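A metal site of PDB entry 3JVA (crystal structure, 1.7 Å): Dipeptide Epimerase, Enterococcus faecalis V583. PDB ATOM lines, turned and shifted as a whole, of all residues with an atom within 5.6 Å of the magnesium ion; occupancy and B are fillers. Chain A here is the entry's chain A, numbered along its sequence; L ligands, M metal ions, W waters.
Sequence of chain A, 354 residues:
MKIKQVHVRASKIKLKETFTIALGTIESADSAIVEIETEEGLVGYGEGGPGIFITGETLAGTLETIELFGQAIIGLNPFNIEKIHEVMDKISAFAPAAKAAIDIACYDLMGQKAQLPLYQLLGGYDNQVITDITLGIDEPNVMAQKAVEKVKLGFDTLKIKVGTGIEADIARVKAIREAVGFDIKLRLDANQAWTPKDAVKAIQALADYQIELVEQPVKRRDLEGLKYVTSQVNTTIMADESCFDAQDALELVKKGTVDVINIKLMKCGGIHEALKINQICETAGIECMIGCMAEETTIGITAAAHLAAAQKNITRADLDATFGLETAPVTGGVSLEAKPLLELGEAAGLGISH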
ATOM      1  N   LYS A 159     -13.922   8.039   4.717  1.00  0.00           N
ATOM      2  CA  LYS A 159     -13.652   9.147   5.612  1.00  0.00           C
ATOM      3  C   LYS A 159     -15.020   9.660   6.054  1.00  0.00           C
ATOM      4  O   LYS A 159     -15.831  10.092   5.230  1.00  0.00           O
ATOM      5  CB  LYS A 159     -12.866  10.247   4.899  1.00  0.00           C
ATOM      6  CG  LYS A 159     -12.619  11.473   5.749  1.00  0.00           C
ATOM      7  CD  LYS A 159     -11.611  12.380   5.065  1.00  0.00           C
ATOM      8  CE  LYS A 159     -11.342  13.636   5.876  1.00  0.00           C
ATOM      9  NZ  LYS A 159     -10.127  14.337   5.368  1.00  0.00           N
ATOM     10  N   LYS A 161     -17.356  12.253   8.125  1.00  0.00           N
ATOM     11  CA  LYS A 161     -17.441  13.588   8.692  1.00  0.00           C
ATOM     12  C   LYS A 161     -18.372  13.559   9.895  1.00  0.00           C
ATOM     13  O   LYS A 161     -19.444  12.958   9.836  1.00  0.00           O
ATOM     14  CB  LYS A 161     -17.970  14.574   7.657  1.00  0.00           C
ATOM     15  CG  LYS A 161     -16.972  14.956   6.574  1.00  0.00           C
ATOM     16  CD  LYS A 161     -15.847  15.806   7.153  1.00  0.00           C
ATOM     17  CE  LYS A 161     -14.895  16.294   6.081  1.00  0.00           C
ATOM     18  NZ  LYS A 161     -13.833  17.176   6.652  1.00  0.00           N
ATOM     19  N   ASP A 189     -13.288  12.682  10.772  1.00  0.00           N
ATOM     20  CA  ASP A 189     -12.869  14.079  10.700  1.00  0.00           C
ATOM     21  C   ASP A 189     -13.930  14.880  11.465  1.00  0.00           C
ATOM     22  O   ASP A 189     -15.078  14.973  11.024  1.00  0.00           O
ATOM     23  CB  ASP A 189     -12.784  14.556   9.247  1.00  0.00           C
ATOM     24  CG  ASP A 189     -12.074  15.893   9.119  1.00  0.00           C
ATOM     25  OD1 ASP A 189     -12.037  16.646  10.113  1.00  0.00           O
ATOM     26  OD2 ASP A 189     -11.559  16.190   8.028  1.00  0.00           O
ATOM     27  N   ASN A 191     -13.542  18.144  12.311  1.00  0.00           N
ATOM     28  CA  ASN A 191     -13.423  19.558  11.985  1.00  0.00           C
ATOM     29  C   ASN A 191     -13.520  20.505  13.192  1.00  0.00           C
ATOM     30  O   ASN A 191     -14.361  21.414  13.207  1.00  0.00           O
ATOM     31  CB  ASN A 191     -14.457  19.954  10.934  1.00  0.00           C
ATOM     32  CG  ASN A 191     -14.050  19.536   9.533  1.00  0.00           C
ATOM     33  OD1 ASN A 191     -14.606  18.593   8.957  1.00  0.00           O
ATOM     34  ND2 ASN A 191     -13.061  20.228   8.972  1.00  0.00           N
ATOM     35  N   GLU A 215      -9.273  12.840  12.667  1.00  0.00           N
ATOM     36  CA  GLU A 215      -8.740  14.091  12.151  1.00  0.00           C
ATOM     37  C   GLU A 215      -9.248  15.330  12.880  1.00  0.00           C
ATOM     38  O   GLU A 215     -10.451  15.470  13.134  1.00  0.00           O
ATOM     39  CB  GLU A 215      -9.084  14.184  10.657  1.00  0.00           C
ATOM     40  CG  GLU A 215      -8.431  15.322   9.892  1.00  0.00           C
ATOM     41  CD  GLU A 215      -8.721  15.251   8.398  1.00  0.00           C
ATOM     42  OE1 GLU A 215      -8.889  14.123   7.878  1.00  0.00           O
ATOM     43  OE2 GLU A 215      -8.772  16.319   7.741  1.00  0.00           O
ATOM     44  N   GLN A 216      -8.314  16.215  13.236  1.00  0.00           N
ATOM     45  CA  GLN A 216      -8.592  17.493  13.894  1.00  0.00           C
ATOM     46  C   GLN A 216      -9.786  17.481  14.849  1.00  0.00           C
ATOM     47  O   GLN A 216     -10.814  18.084  14.577  1.00  0.00           O
ATOM     48  CB  GLN A 216      -8.811  18.579  12.830  1.00  0.00           C
ATOM     49  CG  GLN A 216      -8.650  19.999  13.334  1.00  0.00           C
ATOM     50  CD  GLN A 216      -7.224  20.312  13.741  1.00  0.00           C
ATOM     51  OE1 GLN A 216      -6.276  19.985  13.028  1.00  0.00           O
ATOM     52  NE2 GLN A 216      -7.060  20.969  14.884  1.00  0.00           N
ATOM     53  N   ASP A 240      -5.207  18.724  10.747  1.00  0.00           N
ATOM     54  CA  ASP A 240      -5.571  19.233   9.431  1.00  0.00           C
ATOM     55  C   ASP A 240      -5.470  20.747   9.554  1.00  0.00           C
ATOM     56  O   ASP A 240      -4.432  21.331   9.242  1.00  0.00           O
ATOM     57  CB  ASP A 240      -6.998  18.837   9.047  1.00  0.00           C
ATOM     58  CG  ASP A 240      -7.380  19.324   7.649  1.00  0.00           C
ATOM     59  OD1 ASP A 240      -6.638  20.138   7.064  1.00  0.00           O
ATOM     60  OD2 ASP A 240      -8.435  18.887   7.123  1.00  0.00           O
ATOM     61  N   GLU A 241      -6.528  21.378  10.053  1.00  0.00           N
ATOM     62  CA  GLU A 241      -6.534  22.832  10.206  1.00  0.00           C
ATOM     63  C   GLU A 241      -5.389  23.358  11.081  1.00  0.00           C
ATOM     64  O   GLU A 241      -4.997  24.519  10.940  1.00  0.00           O
ATOM     65  CB  GLU A 241      -7.881  23.319  10.759  1.00  0.00           C
ATOM     66  CG  GLU A 241      -9.024  23.318   9.752  1.00  0.00           C
ATOM     67  CD  GLU A 241      -9.503  21.933   9.349  1.00  0.00           C
ATOM     68  OE1 GLU A 241      -9.177  20.949  10.059  1.00  0.00           O
ATOM     69  OE2 GLU A 241     -10.219  21.820   8.337  1.00  0.00           O
ATOM     70  N   ASN A 262      -2.161  16.176   7.807  1.00  0.00           N
ATOM     71  CA  ASN A 262      -2.851  16.248   6.520  1.00  0.00           C
ATOM     72  C   ASN A 262      -2.315  17.432   5.730  1.00  0.00           C
ATOM     73  O   ASN A 262      -2.457  18.580   6.138  1.00  0.00           O
ATOM     74  CB  ASN A 262      -4.366  16.433   6.736  1.00  0.00           C
ATOM     75  CG  ASN A 262      -5.150  16.430   5.438  1.00  0.00           C
ATOM     76  OD1 ASN A 262      -4.580  16.505   4.349  1.00  0.00           O
ATOM     77  ND2 ASN A 262      -6.473  16.355   5.544  1.00  0.00           N
ATOM     78  N   LYS A 264      -2.321  19.797   2.403  1.00  0.00           N
ATOM     79  CA  LYS A 264      -3.222  20.270   1.350  1.00  0.00           C
ATOM     80  C   LYS A 264      -2.450  21.369   0.623  1.00  0.00           C
ATOM     81  O   LYS A 264      -1.947  22.301   1.256  1.00  0.00           O
ATOM     82  CB  LYS A 264      -4.514  20.847   1.911  1.00  0.00           C
ATOM     83  CG  LYS A 264      -5.493  19.805   2.444  1.00  0.00           C
ATOM     84  CD  LYS A 264      -6.810  20.466   2.821  1.00  0.00           C
ATOM     85  CE  LYS A 264      -7.768  19.455   3.432  1.00  0.00           C
ATOM     86  NZ  LYS A 264      -9.075  20.077   3.787  1.00  0.00           N
HETATM   87  S1  LIG L   1     -11.440  17.506   4.405  1.00  0.00           S
HETATM   88  O1  LIG L   1     -10.510  17.361   5.546  1.00  0.00           O
HETATM   89  O2  LIG L   1     -12.201  16.262   4.229  1.00  0.00           O
HETATM   90  O3  LIG L   1     -10.651  17.784   3.186  1.00  0.00           O
HETATM   91  O4  LIG L   1     -12.365  18.622   4.652  1.00  0.00           O
HETATM   92 MG    MG M   1     -10.012  17.725   7.628  1.00  0.00          MG
HETATM   93  O   HOH W   1     -11.360  19.367   7.260  1.00  0.00           O
HETATM   94  O   HOH W   2     -10.050  18.382   9.610  1.00  0.00           O
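NZ of Lys 159 lies within salt-bridge range of OE1 of Glu 215. The side-chain carboxylate of Glu 215 sits close to the side-chain amide nitrogen of Asn 262 (3.2 Å). The side-chain carboxylate (OD2) of Asp 240 lies close to the side-chain amino group (NZ) of Lys 264 (3.6 Å). N of Asp 240 sits at hydrogen-bond distance from OE1 of Gln 216, 2.8 Å away. NZ of Lys 161 is in salt-bridge range of OD1 of Asp 189, 3.9 Å away. The side-chain amino group (NZ) of Lys 159 sits close to the side-chain carboxylate (OD2) of Asp 189, at 3.5 Å. The side-chain carboxylate (OD1) of Asp 189 is in hydrogen-bond range of the backbone NH (N) of Asn 191 (3.1 Å). The side-chain amino group (NZ) of Lys 161 is in hydrogen-bond range of the side-chain amide oxygen (OD1) of Asn 191 (2.8 Å).
Lys 161 touches the magnesium ion. Of the 10 residues printed, 4 come within 4 Å of the magnesium ion. The nearest printed residue that does not touch the magnesium ion is Lys 159 (4.1 Å).
The side-chain carboxylate (OE2) of Glu 215 is bound to the magnesium ion (1.9 Å). OD2 of Asp 240 is bound to the magnesium ion. Water W2 is bound to the magnesium ion. Water W1 is bound to the magnesium ion. The magnesium ion is bound by O1 of the ligand, at 2.2 Å. The magnesium ion is bound by the side-chain carboxylate (OD2) of Asp 189. The magnesium ion has six donor atoms within binding distance.
Water W2 bridges OD1 of Asp 189 (2.7 Å) and OE1 of Glu 241 (2.7 Å). Water W1 lies within hydrogen-bond range of ND2 of Asn 191 (2.6 Å), OE2 of Glu 241 (2.9 Å) and NZ of Lys 161 (3.4 Å).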
